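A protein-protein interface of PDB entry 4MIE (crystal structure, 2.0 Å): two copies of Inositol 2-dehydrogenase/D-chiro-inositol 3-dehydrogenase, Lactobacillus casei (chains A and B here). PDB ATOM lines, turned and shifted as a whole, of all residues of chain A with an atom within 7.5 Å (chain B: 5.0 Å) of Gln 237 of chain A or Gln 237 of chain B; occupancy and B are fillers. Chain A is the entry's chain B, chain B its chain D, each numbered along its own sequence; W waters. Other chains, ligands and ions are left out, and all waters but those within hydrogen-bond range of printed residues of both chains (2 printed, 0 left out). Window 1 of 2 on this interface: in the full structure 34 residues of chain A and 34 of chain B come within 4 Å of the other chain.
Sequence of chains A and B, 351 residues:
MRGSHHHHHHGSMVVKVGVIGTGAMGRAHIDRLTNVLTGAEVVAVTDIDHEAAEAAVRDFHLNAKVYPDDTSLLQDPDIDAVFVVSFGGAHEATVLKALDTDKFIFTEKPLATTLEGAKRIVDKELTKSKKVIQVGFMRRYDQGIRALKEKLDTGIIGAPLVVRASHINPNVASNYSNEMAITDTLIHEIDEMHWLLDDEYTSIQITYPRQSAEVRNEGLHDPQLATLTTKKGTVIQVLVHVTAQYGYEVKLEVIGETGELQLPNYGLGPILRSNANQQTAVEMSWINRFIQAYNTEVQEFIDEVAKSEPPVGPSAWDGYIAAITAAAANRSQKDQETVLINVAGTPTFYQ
O of Ala 165 of chain B lies within hydrogen-bond range of NH1 of Arg 164 of chain A.
O of Gln 237 of chain B is in hydrogen-bond range of NH2 of Arg 164 of chain A (3.0 Å).
O of Ala 165 of chain A sits at hydrogen-bond distance from NH1 of Arg 164 of chain B.
OG of Ser 166 of chain A sits at hydrogen-bond distance from NH1 of Arg 164 of chain B (3.3 Å).
The backbone carbonyl oxygen of Gln 237 of chain A lies within hydrogen-bond range of the guanidinium group of Arg 164 of chain B, at 2.9 Å.
N of Arg 164 of chain A sits at hydrogen-bond distance from O of Glu 253 of chain A, at 2.9 Å.
The backbone NH of Ala 165 of chain A is in hydrogen-bond range of the backbone carbonyl oxygen of Gln 237 of chain A (3.0 Å).
O of Ser 166 of chain A lies within hydrogen-bond range of N of Lys 251 of chain A.
The backbone NH of Gln 237 of chain B lies within hydrogen-bond range of the backbone carbonyl oxygen of Val 163 of chain B (2.8 Å).
OE1 of Gln 237 of chain B sits at hydrogen-bond distance from NE of Arg 164 of chain B, 3.0 Å away.
O of Gln 237 of chain B sits at hydrogen-bond distance from N of Ala 165 of chain B (3.0 Å).
CB of Leu 239 of chain B touches NH1 of Arg 164 of chain A, 3.8 Å away.
CG1 of Val 235 of chain B touches CD1 of Leu 225 of chain A, at 3.6 Å.
Gln 237 of chain B touches Leu 225 of chain A.
Leu 225 of chain B touches Val 235 of chain A (CD1 to CG1, 3.6 Å).
Gln 237 of chain B touches Gln 237 of chain A (OE1 to OE1, 3.97 Å).
Leu 239 of chain A touches Arg 164 of chain B.
Gln 237 of chain B touches just these residues of chain A: Arg 164 (3.0 Å), Leu 225 (3.8 Å) and Gln 237 (3.97 Å).
Of the printed residues of chain B, Leu 225 of chain A touches Val 235 (3.6 Å) and Gln 237 (3.8 Å).
Of the printed residues of chain B, Val 235 of chain A touches Leu 225 (3.6 Å).
The nearest residue of chain B that does not touch Gln 237 of chain A is Leu 225 of chain B (4.1 Å).
The nearest residue of chain A that does not touch Gln 237 of chain B is Thr 227 of chain A (4.7 Å).
The nearest printed residue of chain A that does not touch Ala 165 of chain B is Gln 237 of chain A (6.9 Å).
Hydrophobic or aromatic side chains of chain A that line the printed part of chain B: Leu 225, Val 235 and Leu 239.
Printed residues of chain B that touch a printed residue of chain A: Arg 164, Ala 165, Leu 225, Val 235, Gln 237 and Leu 239.
Hydrophobic or aromatic side chains of chain B within 4 Å of the printed part of chain A: Leu 225, Val 235 and Leu 239.
Among the printed residues, 11 pairs touch across the chains.
Among the printed residues, no Asp or Glu carboxylate lies within 4 Å of a Lys or Arg side-chain nitrogen of the other chain.
Arg 164 of chain A touches Ala 165 of chain B, and with the chains exchanged Ala 165 of chain A touches Arg 164 of chain B.
Arg 164 of chain A touches Gln 237 of chain B, and with the chains exchanged Gln 237 of chain A touches Arg 164 of chain B.
Arg 164 of chain A touches Leu 239 of chain B, and with the chains exchanged Leu 239 of chain A touches Arg 164 of chain B.
Leu 225 of chain A touches Val 235 of chain B, and with the chains exchanged Val 235 of chain A touches Leu 225 of chain B.
Positions printed for both chains: 162, 163, 164, 165, 225, 226, 227, 235, 236, 237, 238 and 239.
Of the 11 pairs that touch across the chains among the printed residues, 9 have their exchanged pair printed and touching as well.
Water W2 lies within hydrogen-bond range of the side-chain amide nitrogen (NE2) of Gln 237 of chain B (3.0 Å), the backbone carbonyl oxygen (O) of Ala 226 of chain A (3.0 Å), the backbone NH (N) of Val 238 of chain A (3.4 Å) and the side-chain hydroxyl (OG1) of Thr 227 of chain A (3.4 Å).
Water W1 lies within hydrogen-bond range of NE2 of Gln 237 of chain A (3.0 Å), N of Val 238 of chain B (3.2 Å) and O of Ala 226 of chain B (3.2 Å).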
ATOM      1  N   VAL A 162     -19.718   2.436 -23.900  1.00  0.00           N
ATOM      2  CA  VAL A 162     -21.106   2.834 -23.913  1.00  0.00           C
ATOM      3  C   VAL A 162     -21.936   1.877 -23.062  1.00  0.00           C
ATOM      4  O   VAL A 162     -21.664   0.690 -23.016  1.00  0.00           O
ATOM      5  CB  VAL A 162     -21.674   2.860 -25.361  1.00  0.00           C
ATOM      6  CG1 VAL A 162     -23.163   3.201 -25.373  1.00  0.00           C
ATOM      7  CG2 VAL A 162     -20.901   3.806 -26.234  1.00  0.00           C
ATOM      8  N   VAL A 163     -22.941   2.412 -22.386  1.00  0.00           N
ATOM      9  CA  VAL A 163     -23.931   1.606 -21.717  1.00  0.00           C
ATOM     10  C   VAL A 163     -25.317   1.897 -22.280  1.00  0.00           C
ATOM     11  O   VAL A 163     -25.688   3.036 -22.444  1.00  0.00           O
ATOM     12  CB  VAL A 163     -23.968   1.858 -20.209  1.00  0.00           C
ATOM     13  CG1 VAL A 163     -24.976   0.960 -19.549  1.00  0.00           C
ATOM     14  CG2 VAL A 163     -22.615   1.687 -19.600  1.00  0.00           C
ATOM     15  N   ARG A 164     -26.070   0.851 -22.568  1.00  0.00           N
ATOM     16  CA  ARG A 164     -27.452   0.995 -22.978  1.00  0.00           C
ATOM     17  C   ARG A 164     -28.364   0.207 -22.064  1.00  0.00           C
ATOM     18  O   ARG A 164     -28.170  -0.959 -21.855  1.00  0.00           O
ATOM     19  CB  ARG A 164     -27.629   0.567 -24.412  1.00  0.00           C
ATOM     20  CG  ARG A 164     -26.535   1.077 -25.303  1.00  0.00           C
ATOM     21  CD  ARG A 164     -26.761   0.722 -26.706  1.00  0.00           C
ATOM     22  NE  ARG A 164     -27.234   1.879 -27.427  1.00  0.00           N
ATOM     23  CZ  ARG A 164     -27.777   1.838 -28.626  1.00  0.00           C
ATOM     24  NH1 ARG A 164     -27.932   0.681 -29.239  1.00  0.00           N
ATOM     25  NH2 ARG A 164     -28.156   2.951 -29.199  1.00  0.00           N
ATOM     26  N   ALA A 165     -29.349   0.878 -21.507  1.00  0.00           N
ATOM     27  CA  ALA A 165     -30.235   0.277 -20.540  1.00  0.00           C
ATOM     28  C   ALA A 165     -31.683   0.673 -20.776  1.00  0.00           C
ATOM     29  O   ALA A 165     -31.965   1.638 -21.434  1.00  0.00           O
ATOM     30  CB  ALA A 165     -29.816   0.625 -19.142  1.00  0.00           C
ATOM     31  N   SER A 166     -32.576  -0.133 -20.247  1.00  0.00           N
ATOM     32  CA  SER A 166     -33.985   0.136 -20.301  1.00  0.00           C
ATOM     33  C   SER A 166     -34.608  -0.152 -18.940  1.00  0.00           C
ATOM     34  O   SER A 166     -34.262  -1.109 -18.278  1.00  0.00           O
ATOM     35  CB  SER A 166     -34.681  -0.699 -21.387  1.00  0.00           C
ATOM     36  OG  SER A 166     -34.061  -0.603 -22.647  1.00  0.00           O
ATOM     37  N   LEU A 186     -36.001   6.230 -12.832  1.00  0.00           N
ATOM     38  CA  LEU A 186     -34.615   6.410 -13.243  1.00  0.00           C
ATOM     39  C   LEU A 186     -33.609   6.457 -12.087  1.00  0.00           C
ATOM     40  O   LEU A 186     -32.430   6.268 -12.288  1.00  0.00           O
ATOM     41  CB  LEU A 186     -34.471   7.688 -14.077  1.00  0.00           C
ATOM     42  CG  LEU A 186     -33.154   7.949 -14.804  1.00  0.00           C
ATOM     43  CD1 LEU A 186     -32.923   6.902 -15.873  1.00  0.00           C
ATOM     44  CD2 LEU A 186     -33.033   9.339 -15.381  1.00  0.00           C
ATOM     45  N   MET A 193     -25.255   3.047 -12.288  1.00  0.00           N
ATOM     46  CA  MET A 193     -24.246   3.237 -13.322  1.00  0.00           C
ATOM     47  C   MET A 193     -22.864   3.674 -12.836  1.00  0.00           C
ATOM     48  O   MET A 193     -21.866   3.153 -13.290  1.00  0.00           O
ATOM     49  CB  MET A 193     -24.753   4.158 -14.430  1.00  0.00           C
ATOM     50  CG  MET A 193     -25.951   3.636 -15.188  1.00  0.00           C
ATOM     51  SD  MET A 193     -25.721   1.981 -15.811  1.00  0.00           S
ATOM     52  CE  MET A 193     -27.368   1.565 -16.255  1.00  0.00           C
ATOM     53  N   THR A 207     -34.512  13.790 -22.884  1.00  0.00           N
ATOM     54  CA  THR A 207     -35.225  14.128 -24.093  1.00  0.00           C
ATOM     55  C   THR A 207     -36.541  13.387 -24.175  1.00  0.00           C
ATOM     56  O   THR A 207     -36.702  12.332 -23.597  1.00  0.00           O
ATOM     57  CB  THR A 207     -34.373  13.897 -25.362  1.00  0.00           C
ATOM     58  OG1 THR A 207     -33.812  12.592 -25.341  1.00  0.00           O
ATOM     59  CG2 THR A 207     -33.280  14.860 -25.410  1.00  0.00           C
ATOM     60  N   LEU A 225     -35.994   9.546 -22.563  1.00  0.00           N
ATOM     61  CA  LEU A 225     -34.645   9.112 -22.852  1.00  0.00           C
ATOM     62  C   LEU A 225     -33.656   9.908 -22.035  1.00  0.00           C
ATOM     63  O   LEU A 225     -33.629  11.116 -22.101  1.00  0.00           O
ATOM     64  CB  LEU A 225     -34.317   9.285 -24.321  1.00  0.00           C
ATOM     65  CG  LEU A 225     -35.104   8.468 -25.334  1.00  0.00           C
ATOM     66  CD1 LEU A 225     -34.750   8.896 -26.725  1.00  0.00           C
ATOM     67  CD2 LEU A 225     -34.872   6.979 -25.158  1.00  0.00           C
ATOM     68  N   ALA A 226     -32.846   9.219 -21.256  1.00  0.00           N
ATOM     69  CA  ALA A 226     -31.869   9.886 -20.440  1.00  0.00           C
ATOM     70  C   ALA A 226     -30.480   9.561 -20.911  1.00  0.00           C
ATOM     71  O   ALA A 226     -30.122   8.408 -21.055  1.00  0.00           O
ATOM     72  CB  ALA A 226     -32.025   9.481 -19.051  1.00  0.00           C
ATOM     73  N   THR A 227     -29.692  10.588 -21.123  1.00  0.00           N
ATOM     74  CA  THR A 227     -28.341  10.385 -21.552  1.00  0.00           C
ATOM     75  C   THR A 227     -27.399  10.972 -20.518  1.00  0.00           C
ATOM     76  O   THR A 227     -27.460  12.144 -20.219  1.00  0.00           O
ATOM     77  CB  THR A 227     -28.066  10.999 -22.949  1.00  0.00           C
ATOM     78  OG1 THR A 227     -28.871  10.369 -23.935  1.00  0.00           O
ATOM     79  CG2 THR A 227     -26.645  10.812 -23.322  1.00  0.00           C
ATOM     80  N   LEU A 228     -26.547  10.134 -19.965  1.00  0.00           N
ATOM     81  CA  LEU A 228     -25.553  10.576 -19.022  1.00  0.00           C
ATOM     82  C   LEU A 228     -24.149  10.415 -19.587  1.00  0.00           C
ATOM     83  O   LEU A 228     -23.906   9.544 -20.397  1.00  0.00           O
ATOM     84  CB  LEU A 228     -25.652   9.783 -17.730  1.00  0.00           C
ATOM     85  CG  LEU A 228     -26.857   9.856 -16.814  1.00  0.00           C
ATOM     86  CD1 LEU A 228     -27.959   9.010 -17.343  1.00  0.00           C
ATOM     87  CD2 LEU A 228     -26.440   9.406 -15.425  1.00  0.00           C
ATOM     88  N   THR A 234     -17.418   7.447 -20.815  1.00  0.00           N
ATOM     89  CA  THR A 234     -18.473   6.518 -21.110  1.00  0.00           C
ATOM     90  C   THR A 234     -19.799   7.241 -21.296  1.00  0.00           C
ATOM     91  O   THR A 234     -20.123   8.132 -20.542  1.00  0.00           O
ATOM     92  CB  THR A 234     -18.609   5.482 -19.973  1.00  0.00           C
ATOM     93  OG1 THR A 234     -17.375   4.799 -19.815  1.00  0.00           O
ATOM     94  CG2 THR A 234     -19.693   4.488 -20.272  1.00  0.00           C
ATOM     95  N   VAL A 235     -20.561   6.846 -22.297  1.00  0.00           N
ATOM     96  CA  VAL A 235     -21.881   7.403 -22.488  1.00  0.00           C
ATOM     97  C   VAL A 235     -22.945   6.379 -22.147  1.00  0.00           C
ATOM     98  O   VAL A 235     -22.903   5.246 -22.589  1.00  0.00           O
ATOM     99  CB  VAL A 235     -22.068   7.987 -23.909  1.00  0.00           C
ATOM    100  CG1 VAL A 235     -23.484   8.437 -24.116  1.00  0.00           C
ATOM    101  CG2 VAL A 235     -21.126   9.118 -24.134  1.00  0.00           C
ATOM    102  N   ILE A 236     -23.889   6.805 -21.331  1.00  0.00           N
ATOM    103  CA  ILE A 236     -24.959   5.970 -20.879  1.00  0.00           C
ATOM    104  C   ILE A 236     -26.280   6.395 -21.522  1.00  0.00           C
ATOM    105  O   ILE A 236     -26.635   7.540 -21.452  1.00  0.00           O
ATOM    106  CB  ILE A 236     -25.094   6.049 -19.361  1.00  0.00           C
ATOM    107  CG1 ILE A 236     -23.759   5.749 -18.690  1.00  0.00           C
ATOM    108  CG2 ILE A 236     -26.173   5.171 -18.892  1.00  0.00           C
ATOM    109  CD1 ILE A 236     -23.633   6.190 -17.316  1.00  0.00           C
ATOM    110  N   GLN A 237     -26.989   5.462 -22.139  1.00  0.00           N
ATOM    111  CA  GLN A 237     -28.274   5.741 -22.777  1.00  0.00           C
ATOM    112  C   GLN A 237     -29.362   4.911 -22.135  1.00  0.00           C
ATOM    113  O   GLN A 237     -29.423   3.717 -22.330  1.00  0.00           O
ATOM    114  CB  GLN A 237     -28.246   5.456 -24.286  1.00  0.00           C
ATOM    115  CG  GLN A 237     -27.315   6.305 -25.102  1.00  0.00           C
ATOM    116  CD  GLN A 237     -27.410   6.058 -26.593  1.00  0.00           C
ATOM    117  OE1 GLN A 237     -27.595   4.945 -27.035  1.00  0.00           O
ATOM    118  NE2 GLN A 237     -27.283   7.111 -27.364  1.00  0.00           N
ATOM    119  N   VAL A 238     -30.196   5.562 -21.346  1.00  0.00           N
ATOM    120  CA  VAL A 238     -31.295   4.894 -20.681  1.00  0.00           C
ATOM    121  C   VAL A 238     -32.663   5.239 -21.271  1.00  0.00           C
ATOM    122  O   VAL A 238     -33.007   6.381 -21.416  1.00  0.00           O
ATOM    123  CB  VAL A 238     -31.342   5.203 -19.181  1.00  0.00           C
ATOM    124  CG1 VAL A 238     -32.452   4.412 -18.515  1.00  0.00           C
ATOM    125  CG2 VAL A 238     -30.013   4.946 -18.537  1.00  0.00           C
ATOM    126  N   LEU A 239     -33.420   4.216 -21.599  1.00  0.00           N
ATOM    127  CA  LEU A 239     -34.812   4.349 -21.967  1.00  0.00           C
ATOM    128  C   LEU A 239     -35.711   4.147 -20.744  1.00  0.00           C
ATOM    129  O   LEU A 239     -35.685   3.111 -20.112  1.00  0.00           O
ATOM    130  CB  LEU A 239     -35.173   3.312 -23.035  1.00  0.00           C
ATOM    131  CG  LEU A 239     -36.644   3.090 -23.395  1.00  0.00           C
ATOM    132  CD1 LEU A 239     -37.258   4.287 -24.071  1.00  0.00           C
ATOM    133  CD2 LEU A 239     -36.829   1.863 -24.229  1.00  0.00           C
ATOM    134  N   VAL A 240     -36.528   5.140 -20.452  1.00  0.00           N
ATOM    135  CA  VAL A 240     -37.533   5.034 -19.408  1.00  0.00           C
ATOM    136  C   VAL A 240     -38.899   4.960 -20.060  1.00  0.00           C
ATOM    137  O   VAL A 240     -39.298   5.870 -20.751  1.00  0.00           O
ATOM    138  CB  VAL A 240     -37.479   6.216 -18.431  1.00  0.00           C
ATOM    139  CG1 VAL A 240     -38.538   6.069 -17.377  1.00  0.00           C
ATOM    140  CG2 VAL A 240     -36.148   6.319 -17.788  1.00  0.00           C
ATOM    141  N   LYS A 251     -33.299  -3.920 -18.448  1.00  0.00           N
ATOM    142  CA  LYS A 251     -32.313  -4.319 -19.439  1.00  0.00           C
ATOM    143  C   LYS A 251     -31.016  -3.572 -19.220  1.00  0.00           C
ATOM    144  O   LYS A 251     -31.026  -2.424 -18.876  1.00  0.00           O
ATOM    145  CB  LYS A 251     -32.819  -4.042 -20.844  1.00  0.00           C
ATOM    146  CG  LYS A 251     -34.108  -4.715 -21.213  1.00  0.00           C
ATOM    147  CD  LYS A 251     -34.540  -4.304 -22.587  1.00  0.00           C
ATOM    148  CE  LYS A 251     -35.775  -4.988 -23.043  1.00  0.00           C
ATOM    149  NZ  LYS A 251     -35.965  -4.760 -24.466  1.00  0.00           N
ATOM    150  N   GLU A 253     -26.918  -3.434 -20.986  1.00  0.00           N
ATOM    151  CA  GLU A 253     -25.933  -3.824 -21.975  1.00  0.00           C
ATOM    152  C   GLU A 253     -24.720  -2.925 -21.897  1.00  0.00           C
ATOM    153  O   GLU A 253     -24.833  -1.716 -22.002  1.00  0.00           O
ATOM    154  CB  GLU A 253     -26.520  -3.748 -23.375  1.00  0.00           C
ATOM    155  CG  GLU A 253     -25.542  -4.063 -24.483  1.00  0.00           C
ATOM    156  CD  GLU A 253     -26.084  -3.788 -25.882  1.00  0.00           C
ATOM    157  OE1 GLU A 253     -26.923  -2.923 -26.049  1.00  0.00           O
ATOM    158  OE2 GLU A 253     -25.672  -4.459 -26.810  1.00  0.00           O
ATOM    159  N   VAL B 162     -39.580   4.776 -30.130  1.00  0.00           N
ATOM    160  CA  VAL B 162     -38.129   4.792 -30.115  1.00  0.00           C
ATOM    161  C   VAL B 162     -37.632   3.563 -30.876  1.00  0.00           C
ATOM    162  O   VAL B 162     -38.215   2.500 -30.802  1.00  0.00           O
ATOM    163  CB  VAL B 162     -37.559   4.755 -28.676  1.00  0.00           C
ATOM    164  CG1 VAL B 162     -36.047   4.719 -28.667  1.00  0.00           C
ATOM    165  CG2 VAL B 162     -38.063   5.913 -27.851  1.00  0.00           C
ATOM    166  N   VAL B 163     -36.575   3.742 -31.636  1.00  0.00           N
ATOM    167  CA  VAL B 163     -35.873   2.636 -32.231  1.00  0.00           C
ATOM    168  C   VAL B 163     -34.459   2.624 -31.674  1.00  0.00           C
ATOM    169  O   VAL B 163     -33.817   3.640 -31.597  1.00  0.00           O
ATOM    170  CB  VAL B 163     -35.828   2.724 -33.764  1.00  0.00           C
ATOM    171  CG1 VAL B 163     -35.030   1.569 -34.354  1.00  0.00           C
ATOM    172  CG2 VAL B 163     -37.225   2.778 -34.340  1.00  0.00           C
ATOM    173  N   ARG B 164     -34.010   1.464 -31.253  1.00  0.00           N
ATOM    174  CA  ARG B 164     -32.635   1.291 -30.856  1.00  0.00           C
ATOM    175  C   ARG B 164     -31.957   0.241 -31.726  1.00  0.00           C
ATOM    176  O   ARG B 164     -32.473  -0.835 -31.940  1.00  0.00           O
ATOM    177  CB  ARG B 164     -32.540   0.931 -29.397  1.00  0.00           C
ATOM    178  CG  ARG B 164     -33.220   1.907 -28.505  1.00  0.00           C
ATOM    179  CD  ARG B 164     -33.030   1.535 -27.098  1.00  0.00           C
ATOM    180  NE  ARG B 164     -32.301   2.551 -26.381  1.00  0.00           N
ATOM    181  CZ  ARG B 164     -31.891   2.432 -25.133  1.00  0.00           C
ATOM    182  NH1 ARG B 164     -32.135   1.332 -24.461  1.00  0.00           N
ATOM    183  NH2 ARG B 164     -31.239   3.411 -24.573  1.00  0.00           N
ATOM    184  N   ALA B 165     -30.807   0.597 -32.252  1.00  0.00           N
ATOM    185  CA  ALA B 165     -30.114  -0.256 -33.180  1.00  0.00           C
ATOM    186  C   ALA B 165     -28.612  -0.257 -32.939  1.00  0.00           C
ATOM    187  O   ALA B 165     -28.070   0.686 -32.399  1.00  0.00           O
ATOM    188  CB  ALA B 165     -30.410   0.161 -34.580  1.00  0.00           C
ATOM    189  N   LEU B 225     -22.124   7.421 -31.696  1.00  0.00           N
ATOM    190  CA  LEU B 225     -23.543   7.377 -31.452  1.00  0.00           C
ATOM    191  C   LEU B 225     -24.293   8.330 -32.387  1.00  0.00           C
ATOM    192  O   LEU B 225     -23.943   9.475 -32.506  1.00  0.00           O
ATOM    193  CB  LEU B 225     -23.847   7.726 -29.997  1.00  0.00           C
ATOM    194  CG  LEU B 225     -23.179   6.850 -28.958  1.00  0.00           C
ATOM    195  CD1 LEU B 225     -23.224   7.475 -27.624  1.00  0.00           C
ATOM    196  CD2 LEU B 225     -23.865   5.528 -28.929  1.00  0.00           C
ATOM    197  N   ALA B 226     -25.316   7.825 -33.044  1.00  0.00           N
ATOM    198  CA  ALA B 226     -26.134   8.629 -33.926  1.00  0.00           C
ATOM    199  C   ALA B 226     -27.563   8.673 -33.435  1.00  0.00           C
ATOM    200  O   ALA B 226     -28.205   7.654 -33.299  1.00  0.00           O
ATOM    201  CB  ALA B 226     -26.079   8.114 -35.322  1.00  0.00           C
ATOM    202  N   THR B 227     -28.042   9.866 -33.160  1.00  0.00           N
ATOM    203  CA  THR B 227     -29.428  10.046 -32.807  1.00  0.00           C
ATOM    204  C   THR B 227     -30.176  10.767 -33.922  1.00  0.00           C
ATOM    205  O   THR B 227     -29.810  11.846 -34.321  1.00  0.00           O
ATOM    206  CB  THR B 227     -29.581  10.798 -31.486  1.00  0.00           C
ATOM    207  OG1 THR B 227     -28.910  10.099 -30.445  1.00  0.00           O
ATOM    208  CG2 THR B 227     -31.019  10.928 -31.119  1.00  0.00           C
ATOM    209  N   VAL B 235     -37.770   8.669 -32.110  1.00  0.00           N
ATOM    210  CA  VAL B 235     -36.353   8.861 -31.883  1.00  0.00           C
ATOM    211  C   VAL B 235     -35.561   7.588 -32.129  1.00  0.00           C
ATOM    212  O   VAL B 235     -35.851   6.544 -31.579  1.00  0.00           O
ATOM    213  CB  VAL B 235     -36.075   9.397 -30.473  1.00  0.00           C
ATOM    214  CG1 VAL B 235     -34.614   9.560 -30.252  1.00  0.00           C
ATOM    215  CG2 VAL B 235     -36.759  10.712 -30.283  1.00  0.00           C
ATOM    216  N   ILE B 236     -34.555   7.702 -32.967  1.00  0.00           N
ATOM    217  CA  ILE B 236     -33.718   6.600 -33.328  1.00  0.00           C
ATOM    218  C   ILE B 236     -32.326   6.741 -32.702  1.00  0.00           C
ATOM    219  O   ILE B 236     -31.663   7.740 -32.888  1.00  0.00           O
ATOM    220  CB  ILE B 236     -33.600   6.507 -34.837  1.00  0.00           C
ATOM    221  CG1 ILE B 236     -34.981   6.300 -35.468  1.00  0.00           C
ATOM    222  CG2 ILE B 236     -32.664   5.419 -35.229  1.00  0.00           C
ATOM    223  CD1 ILE B 236     -35.208   7.011 -36.759  1.00  0.00           C
ATOM    224  N   GLN B 237     -31.920   5.730 -31.949  1.00  0.00           N
ATOM    225  CA  GLN B 237     -30.597   5.690 -31.342  1.00  0.00           C
ATOM    226  C   GLN B 237     -29.720   4.583 -31.946  1.00  0.00           C
ATOM    227  O   GLN B 237     -29.902   3.424 -31.654  1.00  0.00           O
ATOM    228  CB  GLN B 237     -30.695   5.523 -29.823  1.00  0.00           C
ATOM    229  CG  GLN B 237     -31.318   6.688 -29.052  1.00  0.00           C
ATOM    230  CD  GLN B 237     -31.372   6.470 -27.556  1.00  0.00           C
ATOM    231  OE1 GLN B 237     -31.546   5.370 -27.086  1.00  0.00           O
ATOM    232  NE2 GLN B 237     -31.199   7.530 -26.814  1.00  0.00           N
ATOM    233  N   VAL B 238     -28.778   4.958 -32.796  1.00  0.00           N
ATOM    234  CA  VAL B 238     -27.870   3.995 -33.394  1.00  0.00           C
ATOM    235  C   VAL B 238     -26.477   3.977 -32.763  1.00  0.00           C
ATOM    236  O   VAL B 238     -25.845   4.989 -32.599  1.00  0.00           O
ATOM    237  CB  VAL B 238     -27.690   4.208 -34.890  1.00  0.00           C
ATOM    238  CG1 VAL B 238     -26.874   3.112 -35.465  1.00  0.00           C
ATOM    239  CG2 VAL B 238     -29.005   4.280 -35.581  1.00  0.00           C
ATOM    240  N   LEU B 239     -26.033   2.790 -32.408  1.00  0.00           N
ATOM    241  CA  LEU B 239     -24.659   2.555 -32.026  1.00  0.00           C
ATOM    242  C   LEU B 239     -23.780   2.079 -33.201  1.00  0.00           C
ATOM    243  O   LEU B 239     -24.001   1.035 -33.770  1.00  0.00           O
ATOM    244  CB  LEU B 239     -24.589   1.546 -30.887  1.00  0.00           C
ATOM    245  CG  LEU B 239     -23.204   1.017 -30.530  1.00  0.00           C
ATOM    246  CD1 LEU B 239     -22.360   2.105 -29.955  1.00  0.00           C
ATOM    247  CD2 LEU B 239     -23.278  -0.161 -29.588  1.00  0.00           C
HETATM  248  O   HOH W   1     -27.524   6.604 -30.342  1.00  0.00           O
HETATM  249  O   HOH W   2     -30.988   7.668 -23.869  1.00  0.00           O
